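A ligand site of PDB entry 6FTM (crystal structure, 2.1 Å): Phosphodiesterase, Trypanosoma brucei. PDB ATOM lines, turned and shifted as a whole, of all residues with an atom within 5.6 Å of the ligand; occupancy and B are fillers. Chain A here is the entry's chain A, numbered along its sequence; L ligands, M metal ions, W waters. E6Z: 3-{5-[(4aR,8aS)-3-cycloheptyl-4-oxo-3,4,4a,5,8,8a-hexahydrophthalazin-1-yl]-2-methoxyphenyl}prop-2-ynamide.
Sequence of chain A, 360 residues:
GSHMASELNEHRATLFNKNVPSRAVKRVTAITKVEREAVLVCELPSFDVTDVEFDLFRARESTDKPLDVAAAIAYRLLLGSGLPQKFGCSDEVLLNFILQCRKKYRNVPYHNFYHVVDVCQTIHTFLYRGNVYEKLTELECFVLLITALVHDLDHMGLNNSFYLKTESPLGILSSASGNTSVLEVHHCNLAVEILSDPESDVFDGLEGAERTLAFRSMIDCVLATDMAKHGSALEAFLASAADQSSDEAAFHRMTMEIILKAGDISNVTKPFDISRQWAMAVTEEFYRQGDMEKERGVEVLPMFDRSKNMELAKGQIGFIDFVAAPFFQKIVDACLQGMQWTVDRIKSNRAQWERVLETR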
ATOM      1  N   TYR A 110       3.958  14.044   5.600  1.00  0.00           N
ATOM      2  CA  TYR A 110       2.798  15.011   5.430  1.00  0.00           C
ATOM      3  C   TYR A 110       3.194  16.457   5.027  1.00  0.00           C
ATOM      4  O   TYR A 110       2.624  17.058   4.071  1.00  0.00           O
ATOM      5  CB  TYR A 110       2.008  15.051   6.739  1.00  0.00           C
ATOM      6  CG  TYR A 110       0.744  15.919   6.685  1.00  0.00           C
ATOM      7  CD1 TYR A 110      -0.435  15.427   6.182  1.00  0.00           C
ATOM      8  CD2 TYR A 110       0.763  17.253   7.112  1.00  0.00           C
ATOM      9  CE1 TYR A 110      -1.597  16.237   6.121  1.00  0.00           C
ATOM     10  CE2 TYR A 110      -0.351  18.080   7.052  1.00  0.00           C
ATOM     11  CZ  TYR A 110      -1.543  17.589   6.574  1.00  0.00           C
ATOM     12  OH  TYR A 110      -2.654  18.370   6.557  1.00  0.00           O
ATOM     13  N   HIS A 111       4.118  17.066   5.758  1.00  0.00           N
ATOM     14  CA  HIS A 111       4.453  18.510   5.540  1.00  0.00           C
ATOM     15  C   HIS A 111       5.392  18.763   4.413  1.00  0.00           C
ATOM     16  O   HIS A 111       6.460  19.392   4.602  1.00  0.00           O
ATOM     17  CB  HIS A 111       4.951  19.163   6.827  1.00  0.00           C
ATOM     18  CG  HIS A 111       3.890  19.319   7.842  1.00  0.00           C
ATOM     19  ND1 HIS A 111       3.761  18.448   8.897  1.00  0.00           N
ATOM     20  CD2 HIS A 111       2.862  20.211   7.938  1.00  0.00           C
ATOM     21  CE1 HIS A 111       2.696  18.804   9.612  1.00  0.00           C
ATOM     22  NE2 HIS A 111       2.130  19.862   9.044  1.00  0.00           N
ATOM     23  N   THR A 225      -0.267  30.676  11.521  1.00  0.00           N
ATOM     24  CA  THR A 225      -0.501  29.249  11.336  1.00  0.00           C
ATOM     25  C   THR A 225      -0.016  28.355  12.514  1.00  0.00           C
ATOM     26  O   THR A 225      -0.223  27.121  12.505  1.00  0.00           O
ATOM     27  CB  THR A 225       0.045  28.681  10.020  1.00  0.00           C
ATOM     28  OG1 THR A 225       1.492  28.836   9.893  1.00  0.00           O
ATOM     29  CG2 THR A 225      -0.653  29.362   8.840  1.00  0.00           C
ATOM     30  N   MET A 227      -0.328  26.594  15.722  1.00  0.00           N
ATOM     31  CA  MET A 227      -1.545  26.228  16.462  1.00  0.00           C
ATOM     32  C   MET A 227      -1.605  26.701  17.923  1.00  0.00           C
ATOM     33  O   MET A 227      -2.708  26.811  18.498  1.00  0.00           O
ATOM     34  CB  MET A 227      -1.899  24.750  16.375  1.00  0.00           C
ATOM     35  CG  MET A 227      -2.509  24.330  15.034  1.00  0.00           C
ATOM     36  SD  MET A 227      -4.074  25.078  14.526  1.00  0.00           S
ATOM     37  CE  MET A 227      -5.175  24.128  15.560  1.00  0.00           C
ATOM     38  N   ASP A 264      -5.244  25.367   5.803  1.00  0.00           N
ATOM     39  CA  ASP A 264      -4.285  24.530   6.535  1.00  0.00           C
ATOM     40  C   ASP A 264      -4.896  23.328   7.231  1.00  0.00           C
ATOM     41  O   ASP A 264      -4.274  22.253   7.244  1.00  0.00           O
ATOM     42  CB  ASP A 264      -3.469  25.356   7.546  1.00  0.00           C
ATOM     43  CG  ASP A 264      -2.039  24.776   7.807  1.00  0.00           C
ATOM     44  OD1 ASP A 264      -1.524  24.022   6.939  1.00  0.00           O
ATOM     45  OD2 ASP A 264      -1.480  25.038   8.901  1.00  0.00           O
ATOM     46  N   ILE A 265      -6.100  23.477   7.799  1.00  0.00           N
ATOM     47  CA  ILE A 265      -6.797  22.327   8.423  1.00  0.00           C
ATOM     48  C   ILE A 265      -8.039  21.844   7.612  1.00  0.00           C
ATOM     49  O   ILE A 265      -9.005  21.303   8.189  1.00  0.00           O
ATOM     50  CB  ILE A 265      -7.217  22.618   9.865  1.00  0.00           C
ATOM     51  CG1 ILE A 265      -8.176  23.797   9.932  1.00  0.00           C
ATOM     52  CG2 ILE A 265      -5.968  22.939  10.718  1.00  0.00           C
ATOM     53  CD1 ILE A 265      -8.771  23.985  11.308  1.00  0.00           C
ATOM     54  N   ASN A 267      -8.388  19.267   5.439  1.00  0.00           N
ATOM     55  CA  ASN A 267      -8.377  17.888   4.974  1.00  0.00           C
ATOM     56  C   ASN A 267      -9.763  17.216   5.306  1.00  0.00           C
ATOM     57  O   ASN A 267     -10.256  16.346   4.567  1.00  0.00           O
ATOM     58  CB  ASN A 267      -7.254  17.043   5.650  1.00  0.00           C
ATOM     59  CG  ASN A 267      -5.802  17.515   5.369  1.00  0.00           C
ATOM     60  OD1 ASN A 267      -4.907  17.169   6.145  1.00  0.00           O
ATOM     61  ND2 ASN A 267      -5.560  18.294   4.298  1.00  0.00           N
ATOM     62  N   VAL A 268     -10.368  17.612   6.428  1.00  0.00           N
ATOM     63  CA  VAL A 268     -11.615  17.038   6.855  1.00  0.00           C
ATOM     64  C   VAL A 268     -12.855  17.567   6.112  1.00  0.00           C
ATOM     65  O   VAL A 268     -13.981  17.063   6.361  1.00  0.00           O
ATOM     66  CB  VAL A 268     -11.856  17.199   8.382  1.00  0.00           C
ATOM     67  CG1 VAL A 268     -10.826  16.432   9.150  1.00  0.00           C
ATOM     68  CG2 VAL A 268     -11.924  18.648   8.822  1.00  0.00           C
ATOM     69  N   SER A 275      -9.785  12.515   2.320  1.00  0.00           N
ATOM     70  CA  SER A 275      -9.609  12.889   3.718  1.00  0.00           C
ATOM     71  C   SER A 275      -8.808  11.859   4.501  1.00  0.00           C
ATOM     72  O   SER A 275      -7.881  12.169   5.293  1.00  0.00           O
ATOM     73  CB  SER A 275     -10.988  13.097   4.366  1.00  0.00           C
ATOM     74  OG  SER A 275     -10.904  13.723   5.594  1.00  0.00           O
ATOM     75  N   TRP A 278      -5.035  11.792   3.697  1.00  0.00           N
ATOM     76  CA  TRP A 278      -4.361  12.862   4.454  1.00  0.00           C
ATOM     77  C   TRP A 278      -4.168  12.421   5.932  1.00  0.00           C
ATOM     78  O   TRP A 278      -3.075  12.554   6.499  1.00  0.00           O
ATOM     79  CB  TRP A 278      -5.123  14.211   4.371  1.00  0.00           C
ATOM     80  CG  TRP A 278      -5.027  14.936   3.014  1.00  0.00           C
ATOM     81  CD1 TRP A 278      -6.058  15.267   2.230  1.00  0.00           C
ATOM     82  CD2 TRP A 278      -3.851  15.399   2.344  1.00  0.00           C
ATOM     83  NE1 TRP A 278      -5.615  15.937   1.094  1.00  0.00           N
ATOM     84  CE2 TRP A 278      -4.263  16.005   1.136  1.00  0.00           C
ATOM     85  CE3 TRP A 278      -2.513  15.362   2.623  1.00  0.00           C
ATOM     86  CZ2 TRP A 278      -3.366  16.558   0.232  1.00  0.00           C
ATOM     87  CZ3 TRP A 278      -1.613  15.959   1.696  1.00  0.00           C
ATOM     88  CH2 TRP A 278      -2.047  16.514   0.526  1.00  0.00           C
ATOM     89  N   ALA A 279      -5.222  11.849   6.527  1.00  0.00           N
ATOM     90  CA  ALA A 279      -5.118  11.451   7.931  1.00  0.00           C
ATOM     91  C   ALA A 279      -3.994  10.409   8.213  1.00  0.00           C
ATOM     92  O   ALA A 279      -3.337  10.473   9.255  1.00  0.00           O
ATOM     93  CB  ALA A 279      -6.485  10.935   8.412  1.00  0.00           C
ATOM     94  N   VAL A 282      -0.538  12.363   8.200  1.00  0.00           N
ATOM     95  CA  VAL A 282      -0.282  13.228   9.382  1.00  0.00           C
ATOM     96  C   VAL A 282       0.005  12.409  10.660  1.00  0.00           C
ATOM     97  O   VAL A 282       0.907  12.704  11.456  1.00  0.00           O
ATOM     98  CB  VAL A 282      -1.409  14.321   9.595  1.00  0.00           C
ATOM     99  CG1 VAL A 282      -2.682  13.782  10.151  1.00  0.00           C
ATOM    100  CG2 VAL A 282      -0.910  15.443  10.505  1.00  0.00           C
ATOM    101  N   THR A 283      -0.747  11.357  10.801  1.00  0.00           N
ATOM    102  CA  THR A 283      -0.671  10.385  11.898  1.00  0.00           C
ATOM    103  C   THR A 283       0.726   9.740  11.966  1.00  0.00           C
ATOM    104  O   THR A 283       1.302   9.605  13.037  1.00  0.00           O
ATOM    105  CB  THR A 283      -1.778   9.289  11.697  1.00  0.00           C
ATOM    106  OG1 THR A 283      -3.022   9.870  12.122  1.00  0.00           O
ATOM    107  CG2 THR A 283      -1.552   8.102  12.577  1.00  0.00           C
ATOM    108  N   PHE A 286       3.182  12.304  13.433  1.00  0.00           N
ATOM    109  CA  PHE A 286       3.017  12.273  14.905  1.00  0.00           C
ATOM    110  C   PHE A 286       3.813  11.131  15.584  1.00  0.00           C
ATOM    111  O   PHE A 286       4.513  11.359  16.539  1.00  0.00           O
ATOM    112  CB  PHE A 286       1.509  12.246  15.355  1.00  0.00           C
ATOM    113  CG  PHE A 286       0.733  13.523  15.011  1.00  0.00           C
ATOM    114  CD1 PHE A 286       1.397  14.756  14.664  1.00  0.00           C
ATOM    115  CD2 PHE A 286      -0.655  13.490  14.932  1.00  0.00           C
ATOM    116  CE1 PHE A 286       0.685  15.944  14.317  1.00  0.00           C
ATOM    117  CE2 PHE A 286      -1.373  14.655  14.615  1.00  0.00           C
ATOM    118  CZ  PHE A 286      -0.699  15.881  14.306  1.00  0.00           C
ATOM    119  N   MET A 303      -1.128  10.571  22.121  1.00  0.00           N
ATOM    120  CA  MET A 303      -1.444  10.756  20.715  1.00  0.00           C
ATOM    121  C   MET A 303      -0.210  10.578  19.755  1.00  0.00           C
ATOM    122  O   MET A 303      -0.416  10.316  18.553  1.00  0.00           O
ATOM    123  CB  MET A 303      -2.097  12.157  20.465  1.00  0.00           C
ATOM    124  CG  MET A 303      -2.591  12.321  19.019  1.00  0.00           C
ATOM    125  SD  MET A 303      -3.745  13.668  18.686  1.00  0.00           S
ATOM    126  CE  MET A 303      -2.636  15.018  18.943  1.00  0.00           C
ATOM    127  N   PHE A 304       1.008  10.831  20.256  1.00  0.00           N
ATOM    128  CA  PHE A 304       2.272  10.728  19.502  1.00  0.00           C
ATOM    129  C   PHE A 304       2.967   9.345  19.670  1.00  0.00           C
ATOM    130  O   PHE A 304       4.084   9.109  19.163  1.00  0.00           O
ATOM    131  CB  PHE A 304       3.222  11.878  19.882  1.00  0.00           C
ATOM    132  CG  PHE A 304       2.748  13.270  19.455  1.00  0.00           C
ATOM    133  CD1 PHE A 304       1.705  13.935  20.146  1.00  0.00           C
ATOM    134  CD2 PHE A 304       3.353  13.963  18.373  1.00  0.00           C
ATOM    135  CE1 PHE A 304       1.295  15.230  19.789  1.00  0.00           C
ATOM    136  CE2 PHE A 304       2.935  15.252  17.996  1.00  0.00           C
ATOM    137  CZ  PHE A 304       1.899  15.894  18.691  1.00  0.00           C
ATOM    138  N   LEU A 312      -7.410   4.710  13.207  1.00  0.00           N
ATOM    139  CA  LEU A 312      -7.497   6.079  12.796  1.00  0.00           C
ATOM    140  C   LEU A 312      -8.799   6.744  13.179  1.00  0.00           C
ATOM    141  O   LEU A 312      -8.807   7.927  13.428  1.00  0.00           O
ATOM    142  CB  LEU A 312      -7.336   6.128  11.266  1.00  0.00           C
ATOM    143  CG  LEU A 312      -6.758   7.329  10.568  1.00  0.00           C
ATOM    144  CD1 LEU A 312      -5.774   8.124  11.454  1.00  0.00           C
ATOM    145  CD2 LEU A 312      -6.050   6.890   9.294  1.00  0.00           C
ATOM    146  N   GLY A 315      -9.227   9.230  16.391  1.00  0.00           N
ATOM    147  CA  GLY A 315      -8.384  10.392  16.256  1.00  0.00           C
ATOM    148  C   GLY A 315      -9.004  11.438  15.353  1.00  0.00           C
ATOM    149  O   GLY A 315      -8.958  12.582  15.633  1.00  0.00           O
ATOM    150  N   GLN A 316      -9.562  10.999  14.257  1.00  0.00           N
ATOM    151  CA  GLN A 316     -10.215  11.900  13.327  1.00  0.00           C
ATOM    152  C   GLN A 316     -11.516  12.479  13.915  1.00  0.00           C
ATOM    153  O   GLN A 316     -11.806  13.651  13.723  1.00  0.00           O
ATOM    154  CB  GLN A 316     -10.449  11.247  11.956  1.00  0.00           C
ATOM    155  CG  GLN A 316      -9.122  11.070  11.149  1.00  0.00           C
ATOM    156  CD  GLN A 316      -8.485  12.392  10.720  1.00  0.00           C
ATOM    157  OE1 GLN A 316      -8.950  13.015   9.772  1.00  0.00           O
ATOM    158  NE2 GLN A 316      -7.408  12.827  11.420  1.00  0.00           N
ATOM    159  N   PHE A 319     -10.346  15.155  16.397  1.00  0.00           N
ATOM    160  CA  PHE A 319      -9.882  16.368  15.669  1.00  0.00           C
ATOM    161  C   PHE A 319     -11.099  17.167  15.170  1.00  0.00           C
ATOM    162  O   PHE A 319     -11.185  18.386  15.383  1.00  0.00           O
ATOM    163  CB  PHE A 319      -9.020  15.996  14.460  1.00  0.00           C
ATOM    164  CG  PHE A 319      -8.451  17.195  13.701  1.00  0.00           C
ATOM    165  CD1 PHE A 319      -7.548  18.032  14.301  1.00  0.00           C
ATOM    166  CD2 PHE A 319      -8.845  17.474  12.386  1.00  0.00           C
ATOM    167  CE1 PHE A 319      -7.028  19.130  13.632  1.00  0.00           C
ATOM    168  CE2 PHE A 319      -8.298  18.548  11.684  1.00  0.00           C
ATOM    169  CZ  PHE A 319      -7.413  19.396  12.322  1.00  0.00           C
ATOM    170  N   VAL A 323     -11.504  20.577  17.396  1.00  0.00           N
ATOM    171  CA  VAL A 323     -10.832  21.623  16.634  1.00  0.00           C
ATOM    172  C   VAL A 323     -11.593  22.067  15.396  1.00  0.00           C
ATOM    173  O   VAL A 323     -12.024  23.189  15.340  1.00  0.00           O
ATOM    174  CB  VAL A 323      -9.459  21.140  16.137  1.00  0.00           C
ATOM    175  CG1 VAL A 323      -8.736  22.304  15.414  1.00  0.00           C
ATOM    176  CG2 VAL A 323      -8.632  20.621  17.332  1.00  0.00           C
HETATM  177  C1  E6Z L   1      -6.216  15.427   9.346  1.00  0.00           C
HETATM  178  C10 E6Z L   1      -5.580  12.537  14.551  1.00  0.00           C
HETATM  179  C11 E6Z L   1      -2.836  19.207  13.434  1.00  0.00           C
HETATM  180  C12 E6Z L   1      -2.433  20.175  16.868  1.00  0.00           C
HETATM  181  C13 E6Z L   1      -2.113  18.813  17.501  1.00  0.00           C
HETATM  182  C14 E6Z L   1      -1.920  18.785  19.012  1.00  0.00           C
HETATM  183  C15 E6Z L   1      -3.217  19.060  19.701  1.00  0.00           C
HETATM  184  C16 E6Z L   1      -3.603  20.498  19.690  1.00  0.00           C
HETATM  185  C17 E6Z L   1      -4.350  20.967  18.475  1.00  0.00           C
HETATM  186  C18 E6Z L   1      -3.854  20.620  17.075  1.00  0.00           C
HETATM  187  C19 E6Z L   1      -1.045  20.807  14.876  1.00  0.00           C
HETATM  188  C2  E6Z L   1      -5.151  16.268  11.333  1.00  0.00           C
HETATM  189  C20 E6Z L   1      -0.691  20.502  13.439  1.00  0.00           C
HETATM  190  C21 E6Z L   1       0.194  21.584  12.783  1.00  0.00           C
HETATM  191  C22 E6Z L   1      -0.592  22.738  12.261  1.00  0.00           C
HETATM  192  C23 E6Z L   1      -1.910  22.735  12.106  1.00  0.00           C
HETATM  193  C24 E6Z L   1      -2.785  21.570  12.449  1.00  0.00           C
HETATM  194  C25 E6Z L   1      -1.998  20.241  12.665  1.00  0.00           C
HETATM  195  C3  E6Z L   1      -4.726  17.420  10.700  1.00  0.00           C
HETATM  196  C4  E6Z L   1      -3.967  18.360  11.379  1.00  0.00           C
HETATM  197  C5  E6Z L   1      -3.629  18.176  12.716  1.00  0.00           C
HETATM  198  C6  E6Z L   1      -4.052  17.012  13.367  1.00  0.00           C
HETATM  199  C7  E6Z L   1      -4.814  16.051  12.696  1.00  0.00           C
HETATM  200  C8  E6Z L   1      -5.196  14.842  13.371  1.00  0.00           C
HETATM  201  C9  E6Z L   1      -5.421  13.810  13.939  1.00  0.00           C
HETATM  202  N1  E6Z L   1      -5.052  12.334  15.791  1.00  0.00           N
HETATM  203  N2  E6Z L   1      -2.890  19.208  14.722  1.00  0.00           N
HETATM  204  N3  E6Z L   1      -2.124  20.102  15.423  1.00  0.00           N
HETATM  205  O1  E6Z L   1      -5.886  15.282  10.734  1.00  0.00           O
HETATM  206  O2  E6Z L   1      -6.232  11.719  13.918  1.00  0.00           O
HETATM  207  O3  E6Z L   1      -0.410  21.617  15.533  1.00  0.00           O
HETATM  208 MG    MG M   1       2.850  24.995   9.570  1.00  0.00          MG
HETATM  209  O   HOH W   1      -8.627  14.229   7.177  1.00  0.00           O
HETATM  210  O   HOH W   2       3.552  22.040  12.419  1.00  0.00           O
HETATM  211  O   HOH W   3      -3.726  19.899   8.382  1.00  0.00           O
HETATM  212  O   HOH W   4       1.204  24.327  15.047  1.00  0.00           O
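An oxygen (O2) of the ligand sits at hydrogen-bond distance from the backbone NH of Gln 316 (3.4 Å).
NE2 of Gln 316 lies within hydrogen-bond range of O1 of the ligand (3.0 Å).
A nitrogen (N1) of the ligand sits at hydrogen-bond distance from the side-chain sulfur (SD) of Met 303.
OD1 of Asn 267 lies within hydrogen-bond range of OH of Tyr 110 (2.6 Å).
The backbone carbonyl oxygen of Asn 267 lies within hydrogen-bond range of the side-chain hydroxyl of Ser 275 (2.9 Å).
The backbone carbonyl oxygen of Gly 315 lies close to an oxygen (O2) of the ligand (3.3 Å).
Residues that only touch the ligand: Met 227 (3.4 Å), Asp 264 (3.97 Å), Ile 265 (3.9 Å), Asn 267 (3.9 Å), Val 282 (3.6 Å), Phe 286 (3.7 Å) and Phe 319 (3.6 Å).
Hydrophobic or aromatic side chains that line the ligand: Met 227, Ile 265, Val 282, Phe 286, Met 303 and Phe 319.
Ten residues have an atom within 4 Å of the ligand: Met 227, Asp 264, Ile 265, Asn 267, Val 282, Phe 286, Met 303, Gly 315, Gln 316 and Phe 319.
Water W4 bridges N of Met 227 (2.8 Å) and O3 of the ligand (3.2 Å).
Water W3 bridges OH of Tyr 110 and O of Asp 264.
Water W1 bridges the side-chain hydroxyl of Ser 275 (2.8 Å) and the side-chain amide oxygen of Gln 316 (2.9 Å).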
